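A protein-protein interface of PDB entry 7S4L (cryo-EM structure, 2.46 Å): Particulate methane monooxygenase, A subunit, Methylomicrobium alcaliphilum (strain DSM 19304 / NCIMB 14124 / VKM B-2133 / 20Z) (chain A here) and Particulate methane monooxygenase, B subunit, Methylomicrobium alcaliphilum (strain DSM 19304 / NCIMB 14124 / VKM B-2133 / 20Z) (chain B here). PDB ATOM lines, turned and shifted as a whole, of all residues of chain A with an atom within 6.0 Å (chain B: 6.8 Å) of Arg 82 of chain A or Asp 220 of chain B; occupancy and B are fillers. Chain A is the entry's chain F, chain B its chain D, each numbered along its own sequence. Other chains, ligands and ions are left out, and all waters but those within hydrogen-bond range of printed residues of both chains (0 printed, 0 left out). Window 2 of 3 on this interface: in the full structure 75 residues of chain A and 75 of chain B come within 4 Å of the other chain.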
ATOM      1  N   ALA A  77      22.452  -7.224 -30.151  1.00  0.00           N
ATOM      2  CA  ALA A  77      23.845  -7.188 -30.656  1.00  0.00           C
ATOM      3  C   ALA A  77      24.323  -5.752 -30.910  1.00  0.00           C
ATOM      4  O   ALA A  77      25.534  -5.585 -31.144  1.00  0.00           O
ATOM      5  CB  ALA A  77      23.972  -8.046 -31.882  1.00  0.00           C
ATOM      6  N   VAL A  78      23.425  -4.760 -30.931  1.00  0.00           N
ATOM      7  CA  VAL A  78      23.892  -3.342 -31.064  1.00  0.00           C
ATOM      8  C   VAL A  78      23.287  -2.506 -29.937  1.00  0.00           C
ATOM      9  O   VAL A  78      23.877  -1.469 -29.591  1.00  0.00           O
ATOM     10  CB  VAL A  78      23.619  -2.707 -32.442  1.00  0.00           C
ATOM     11  CG1 VAL A  78      23.872  -3.663 -33.594  1.00  0.00           C
ATOM     12  CG2 VAL A  78      22.249  -2.059 -32.532  1.00  0.00           C
ATOM     13  N   LEU A  79      22.173  -2.955 -29.360  1.00  0.00           N
ATOM     14  CA  LEU A  79      21.614  -2.225 -28.195  1.00  0.00           C
ATOM     15  C   LEU A  79      22.313  -2.746 -26.941  1.00  0.00           C
ATOM     16  O   LEU A  79      21.595  -3.100 -26.003  1.00  0.00           O
ATOM     17  CB  LEU A  79      20.100  -2.447 -28.127  1.00  0.00           C
ATOM     18  CG  LEU A  79      19.254  -1.183 -28.264  1.00  0.00           C
ATOM     19  CD1 LEU A  79      19.694  -0.361 -29.462  1.00  0.00           C
ATOM     20  CD2 LEU A  79      17.776  -1.520 -28.358  1.00  0.00           C
ATOM     21  N   TRP A  80      23.647  -2.831 -26.962  1.00  0.00           N
ATOM     22  CA  TRP A  80      24.440  -3.278 -25.788  1.00  0.00           C
ATOM     23  C   TRP A  80      25.909  -2.893 -25.990  1.00  0.00           C
ATOM     24  O   TRP A  80      26.539  -2.463 -25.021  1.00  0.00           O
ATOM     25  CB  TRP A  80      24.284  -4.776 -25.503  1.00  0.00           C
ATOM     26  CG  TRP A  80      23.620  -4.987 -24.181  1.00  0.00           C
ATOM     27  CD1 TRP A  80      22.392  -5.534 -23.953  1.00  0.00           C
ATOM     28  CD2 TRP A  80      24.123  -4.572 -22.900  1.00  0.00           C
ATOM     29  NE1 TRP A  80      22.110  -5.526 -22.613  1.00  0.00           N
ATOM     30  CE2 TRP A  80      23.152  -4.936 -21.946  1.00  0.00           C
ATOM     31  CE3 TRP A  80      25.300  -3.959 -22.462  1.00  0.00           C
ATOM     32  CZ2 TRP A  80      23.323  -4.679 -20.591  1.00  0.00           C
ATOM     33  CZ3 TRP A  80      25.470  -3.713 -21.119  1.00  0.00           C
ATOM     34  CH2 TRP A  80      24.492  -4.071 -20.197  1.00  0.00           C
ATOM     35  N   TRP A  81      26.444  -3.069 -27.195  1.00  0.00           N
ATOM     36  CA  TRP A  81      27.888  -2.763 -27.357  1.00  0.00           C
ATOM     37  C   TRP A  81      28.043  -1.376 -27.985  1.00  0.00           C
ATOM     38  O   TRP A  81      29.193  -0.929 -28.145  1.00  0.00           O
ATOM     39  CB  TRP A  81      28.626  -3.860 -28.136  1.00  0.00           C
ATOM     40  CG  TRP A  81      28.030  -5.232 -28.032  1.00  0.00           C
ATOM     41  CD1 TRP A  81      27.611  -6.004 -29.073  1.00  0.00           C
ATOM     42  CD2 TRP A  81      27.814  -6.018 -26.845  1.00  0.00           C
ATOM     43  NE1 TRP A  81      27.122  -7.198 -28.622  1.00  0.00           N
ATOM     44  CE2 TRP A  81      27.237  -7.239 -27.260  1.00  0.00           C
ATOM     45  CE3 TRP A  81      28.036  -5.816 -25.478  1.00  0.00           C
ATOM     46  CZ2 TRP A  81      26.887  -8.245 -26.361  1.00  0.00           C
ATOM     47  CZ3 TRP A  81      27.682  -6.806 -24.591  1.00  0.00           C
ATOM     48  CH2 TRP A  81      27.124  -8.005 -25.029  1.00  0.00           C
ATOM     49  N   ARG A  82      26.923  -0.721 -28.307  1.00  0.00           N
ATOM     50  CA  ARG A  82      26.982   0.656 -28.864  1.00  0.00           C
ATOM     51  C   ARG A  82      26.466   1.644 -27.816  1.00  0.00           C
ATOM     52  O   ARG A  82      27.033   2.750 -27.731  1.00  0.00           O
ATOM     53  CB  ARG A  82      26.145   0.778 -30.141  1.00  0.00           C
ATOM     54  CG  ARG A  82      26.812   0.254 -31.404  1.00  0.00           C
ATOM     55  CD  ARG A  82      28.325   0.352 -31.372  1.00  0.00           C
ATOM     56  NE  ARG A  82      28.855   1.525 -32.048  1.00  0.00           N
ATOM     57  CZ  ARG A  82      29.576   2.469 -31.455  1.00  0.00           C
ATOM     58  NH1 ARG A  82      30.026   3.498 -32.153  1.00  0.00           N
ATOM     59  NH2 ARG A  82      29.848   2.382 -30.164  1.00  0.00           N
ATOM     60  N   TYR A  83      25.430   1.267 -27.059  1.00  0.00           N
ATOM     61  CA  TYR A  83      24.819   2.222 -26.095  1.00  0.00           C
ATOM     62  C   TYR A  83      24.599   1.568 -24.728  1.00  0.00           C
ATOM     63  O   TYR A  83      23.867   2.161 -23.922  1.00  0.00           O
ATOM     64  CB  TYR A  83      23.455   2.708 -26.593  1.00  0.00           C
ATOM     65  CG  TYR A  83      23.345   2.955 -28.074  1.00  0.00           C
ATOM     66  CD1 TYR A  83      22.651   2.084 -28.898  1.00  0.00           C
ATOM     67  CD2 TYR A  83      23.925   4.071 -28.651  1.00  0.00           C
ATOM     68  CE1 TYR A  83      22.548   2.308 -30.260  1.00  0.00           C
ATOM     69  CE2 TYR A  83      23.836   4.305 -30.011  1.00  0.00           C
ATOM     70  CZ  TYR A  83      23.144   3.423 -30.818  1.00  0.00           C
ATOM     71  OH  TYR A  83      23.047   3.669 -32.156  1.00  0.00           O
ATOM     72  N   ARG A  84      25.163   0.378 -24.497  1.00  0.00           N
ATOM     73  CA  ARG A  84      25.031  -0.317 -23.185  1.00  0.00           C
ATOM     74  C   ARG A  84      23.564  -0.354 -22.743  1.00  0.00           C
ATOM     75  O   ARG A  84      23.312  -0.176 -21.539  1.00  0.00           O
ATOM     76  CB  ARG A  84      25.916   0.348 -22.127  1.00  0.00           C
ATOM     77  CG  ARG A  84      27.042  -0.534 -21.617  1.00  0.00           C
ATOM     78  CD  ARG A  84      28.112  -0.734 -22.671  1.00  0.00           C
ATOM     79  NE  ARG A  84      29.254  -1.456 -22.138  1.00  0.00           N
ATOM     80  CZ  ARG A  84      29.695  -2.613 -22.610  1.00  0.00           C
ATOM     81  NH1 ARG A  84      30.746  -3.197 -22.061  1.00  0.00           N
ATOM     82  NH2 ARG A  84      29.083  -3.183 -23.632  1.00  0.00           N
ATOM     83  N   GLU A 241      27.344  -0.082 -40.481  1.00  0.00           N
ATOM     84  CA  GLU A 241      27.222   1.255 -41.040  1.00  0.00           C
ATOM     85  C   GLU A 241      27.896   1.370 -42.398  1.00  0.00           C
ATOM     86  O   GLU A 241      28.159   2.482 -42.863  1.00  0.00           O
ATOM     87  CB  GLU A 241      27.808   2.281 -40.077  1.00  0.00           C
ATOM     88  CG  GLU A 241      27.110   2.325 -38.744  1.00  0.00           C
ATOM     89  CD  GLU A 241      27.952   2.986 -37.680  1.00  0.00           C
ATOM     90  OE1 GLU A 241      28.853   2.318 -37.138  1.00  0.00           O
ATOM     91  OE2 GLU A 241      27.720   4.175 -37.386  1.00  0.00           O
ATOM     92  N   PHE B 212      20.275   6.794 -25.685  1.00  0.00           N
ATOM     93  CA  PHE B 212      20.781   7.057 -27.062  1.00  0.00           C
ATOM     94  C   PHE B 212      21.976   8.018 -27.064  1.00  0.00           C
ATOM     95  O   PHE B 212      23.093   7.539 -26.800  1.00  0.00           O
ATOM     96  CB  PHE B 212      19.645   7.463 -28.008  1.00  0.00           C
ATOM     97  CG  PHE B 212      18.521   6.463 -28.092  1.00  0.00           C
ATOM     98  CD1 PHE B 212      17.215   6.839 -27.829  1.00  0.00           C
ATOM     99  CD2 PHE B 212      18.769   5.141 -28.425  1.00  0.00           C
ATOM    100  CE1 PHE B 212      16.180   5.920 -27.898  1.00  0.00           C
ATOM    101  CE2 PHE B 212      17.734   4.221 -28.494  1.00  0.00           C
ATOM    102  CZ  PHE B 212      16.443   4.612 -28.232  1.00  0.00           C
ATOM    103  N   ARG B 215      24.630   7.943 -24.226  1.00  0.00           N
ATOM    104  CA  ARG B 215      25.167   6.559 -24.211  1.00  0.00           C
ATOM    105  C   ARG B 215      26.105   6.359 -25.406  1.00  0.00           C
ATOM    106  O   ARG B 215      27.200   5.828 -25.193  1.00  0.00           O
ATOM    107  CB  ARG B 215      24.015   5.551 -24.193  1.00  0.00           C
ATOM    108  CG  ARG B 215      22.832   6.001 -23.349  1.00  0.00           C
ATOM    109  CD  ARG B 215      22.249   4.876 -22.521  1.00  0.00           C
ATOM    110  NE  ARG B 215      23.260   4.178 -21.739  1.00  0.00           N
ATOM    111  CZ  ARG B 215      23.027   3.092 -21.012  1.00  0.00           C
ATOM    112  NH1 ARG B 215      21.814   2.569 -20.971  1.00  0.00           N
ATOM    113  NH2 ARG B 215      24.010   2.527 -20.336  1.00  0.00           N
ATOM    114  N   ARG B 216      25.697   6.782 -26.605  1.00  0.00           N
ATOM    115  CA  ARG B 216      26.581   6.685 -27.796  1.00  0.00           C
ATOM    116  C   ARG B 216      27.909   7.378 -27.478  1.00  0.00           C
ATOM    117  O   ARG B 216      28.944   6.700 -27.547  1.00  0.00           O
ATOM    118  CB  ARG B 216      25.919   7.325 -29.021  1.00  0.00           C
ATOM    119  CG  ARG B 216      26.789   7.331 -30.267  1.00  0.00           C
ATOM    120  CD  ARG B 216      26.917   5.974 -30.932  1.00  0.00           C
ATOM    121  NE  ARG B 216      27.313   6.101 -32.328  1.00  0.00           N
ATOM    122  CZ  ARG B 216      26.833   5.361 -33.321  1.00  0.00           C
ATOM    123  NH1 ARG B 216      25.931   4.427 -33.075  1.00  0.00           N
ATOM    124  NH2 ARG B 216      27.255   5.556 -34.556  1.00  0.00           N
ATOM    125  N   ILE B 217      27.855   8.677 -27.158  1.00  0.00           N
ATOM    126  CA  ILE B 217      29.084   9.477 -26.872  1.00  0.00           C
ATOM    127  C   ILE B 217      29.933   8.742 -25.832  1.00  0.00           C
ATOM    128  O   ILE B 217      31.150   8.633 -26.048  1.00  0.00           O
ATOM    129  CB  ILE B 217      28.692  10.897 -26.414  1.00  0.00           C
ATOM    130  CG1 ILE B 217      27.953  11.659 -27.517  1.00  0.00           C
ATOM    131  CG2 ILE B 217      29.896  11.675 -25.908  1.00  0.00           C
ATOM    132  CD1 ILE B 217      27.318  12.947 -27.051  1.00  0.00           C
ATOM    133  N   ALA B 218      29.310   8.235 -24.765  1.00  0.00           N
ATOM    134  CA  ALA B 218      30.063   7.560 -23.683  1.00  0.00           C
ATOM    135  C   ALA B 218      30.904   6.417 -24.260  1.00  0.00           C
ATOM    136  O   ALA B 218      32.132   6.470 -24.114  1.00  0.00           O
ATOM    137  CB  ALA B 218      29.120   7.072 -22.615  1.00  0.00           C
ATOM    138  N   VAL B 219      30.273   5.429 -24.901  1.00  0.00           N
ATOM    139  CA  VAL B 219      31.046   4.248 -25.392  1.00  0.00           C
ATOM    140  C   VAL B 219      31.999   4.679 -26.514  1.00  0.00           C
ATOM    141  O   VAL B 219      33.097   4.097 -26.605  1.00  0.00           O
ATOM    142  CB  VAL B 219      30.137   3.078 -25.818  1.00  0.00           C
ATOM    143  CG1 VAL B 219      30.873   1.752 -25.712  1.00  0.00           C
ATOM    144  CG2 VAL B 219      28.859   3.024 -24.998  1.00  0.00           C
ATOM    145  N   ASP B 220      31.610   5.672 -27.320  1.00  0.00           N
ATOM    146  CA  ASP B 220      32.503   6.187 -28.393  1.00  0.00           C
ATOM    147  C   ASP B 220      33.787   6.737 -27.763  1.00  0.00           C
ATOM    148  O   ASP B 220      34.870   6.473 -28.316  1.00  0.00           O
ATOM    149  CB  ASP B 220      31.807   7.250 -29.245  1.00  0.00           C
ATOM    150  CG  ASP B 220      30.800   6.675 -30.227  1.00  0.00           C
ATOM    151  OD1 ASP B 220      30.533   5.460 -30.150  1.00  0.00           O
ATOM    152  OD2 ASP B 220      30.287   7.451 -31.058  1.00  0.00           O
ATOM    153  N   ALA B 221      33.666   7.466 -26.648  1.00  0.00           N
ATOM    154  CA  ALA B 221      34.846   8.037 -25.960  1.00  0.00           C
ATOM    155  C   ALA B 221      35.625   6.925 -25.250  1.00  0.00           C
ATOM    156  O   ALA B 221      36.855   7.063 -25.114  1.00  0.00           O
ATOM    157  CB  ALA B 221      34.406   9.105 -24.990  1.00  0.00           C
ATOM    158  N   GLY B 222      34.934   5.869 -24.812  1.00  0.00           N
ATOM    159  CA  GLY B 222      35.594   4.755 -24.107  1.00  0.00           C
ATOM    160  C   GLY B 222      35.044   4.593 -22.703  1.00  0.00           C
ATOM    161  O   GLY B 222      35.570   3.749 -21.956  1.00  0.00           O
ATOM    162  N   LYS B 223      34.012   5.368 -22.359  1.00  0.00           N
ATOM    163  CA  LYS B 223      33.341   5.199 -21.045  1.00  0.00           C
ATOM    164  C   LYS B 223      32.207   4.191 -21.243  1.00  0.00           C
ATOM    165  O   LYS B 223      31.039   4.577 -21.048  1.00  0.00           O
ATOM    166  CB  LYS B 223      32.815   6.544 -20.537  1.00  0.00           C
ATOM    167  CG  LYS B 223      33.467   7.769 -21.163  1.00  0.00           C
ATOM    168  CD  LYS B 223      34.412   8.494 -20.227  1.00  0.00           C
ATOM    169  CE  LYS B 223      35.870   8.172 -20.479  1.00  0.00           C
ATOM    170  NZ  LYS B 223      36.160   8.015 -21.923  1.00  0.00           N
ATOM    171  N   ALA B 224      32.545   2.953 -21.623  1.00  0.00           N
ATOM    172  CA  ALA B 224      31.530   1.899 -21.862  1.00  0.00           C
ATOM    173  C   ALA B 224      30.609   1.774 -20.647  1.00  0.00           C
ATOM    174  O   ALA B 224      29.414   1.488 -20.850  1.00  0.00           O
ATOM    175  CB  ALA B 224      32.218   0.593 -22.170  1.00  0.00           C
ATOM    176  N   SER B 226      28.423   3.329 -18.976  1.00  0.00           N
ATOM    177  CA  SER B 226      27.615   4.573 -19.058  1.00  0.00           C
ATOM    178  C   SER B 226      26.665   4.645 -17.861  1.00  0.00           C
ATOM    179  O   SER B 226      26.861   5.525 -17.002  1.00  0.00           O
ATOM    180  CB  SER B 226      26.869   4.647 -20.364  1.00  0.00           C
ATOM    181  OG  SER B 226      27.046   3.455 -21.116  1.00  0.00           O
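Hydrophobic or aromatic side chains of chain B within 4 Å of the printed part of chain A: Val 219 and Ala 224. Along chain B the printed residues that touch a printed residue of chain A span positions 215 to 226. Hydrophobic or aromatic side chains of chain A that line the printed part of chain B: Tyr 83. Among the printed residues, 11 pairs touch across the chains.
Among the printed residues, merely in contact across the chains: Trp 81 of chain A with Val 219 of chain B, Arg 82 of chain A with Arg 215 of chain B, Arg 82 of chain A with Arg 216 of chain B, Arg 82 of chain A with Val 219 of chain B and Arg 84 of chain A with Ser 226 of chain B.
Printed residues of chain B within 4 Å of Glu 241 of chain A: Arg 216 (3.2 Å). Phe 212 of chain B touches none of the printed residues of chain A. Printed residues of chain A within 4 Å of Arg 215 of chain B: Arg 82, Tyr 83 and Arg 84. Asp 220 of chain B touches one residue of chain A. Ala 221 of chain B touches none of the printed residues of chain A. Of the printed residues of chain A, Ser 226 of chain B touches Arg 84 (3.5 Å). The nearest printed residue of chain A that does not touch Asp 220 of chain B is Tyr 83 of chain A (6.8 Å).
The side-chain hydroxyl of Ser 226 of chain B is in hydrogen-bond range of the backbone carbonyl oxygen of Ala 224 of chain B (3.1 Å). NE1 of Trp 81 of chain A sits close to O of Ala 77 of chain A (3.4 Å). The backbone carbonyl oxygen of Trp 80 of chain A sits at hydrogen-bond distance from the guanidinium group of Arg 84 of chain A (3.0 Å). OD2 of Asp 220 of chain B lies within salt-bridge range of NE of Arg 216 of chain B, 3.5 Å away. The guanidinium group (NH2) of Arg 215 of chain B is in hydrogen-bond range of the side-chain hydroxyl (OG) of Ser 226 of chain B (3.3 Å).
O of Arg 84 of chain A sits at hydrogen-bond distance from NH2 of Arg 215 of chain B (3.0 Å). The guanidinium group (NH2) of Arg 216 of chain B lies within salt-bridge range of the side-chain carboxylate (OE2) of Glu 241 of chain A (3.2 Å). The guanidinium group of Arg 216 of chain B is in hydrogen-bond range of the side-chain hydroxyl of Tyr 83 of chain A (3.1 Å). The side-chain carboxylate of Asp 220 of chain B lies within salt-bridge range of the guanidinium group of Arg 82 of chain A, 2.8 Å away. NE of Arg 84 of chain A sits close to O of Ala 224 of chain B (3.2 Å). The backbone carbonyl oxygen (O) of Tyr 83 of chain A sits at hydrogen-bond distance from the guanidinium group (NE) of Arg 215 of chain B (3.0 Å).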
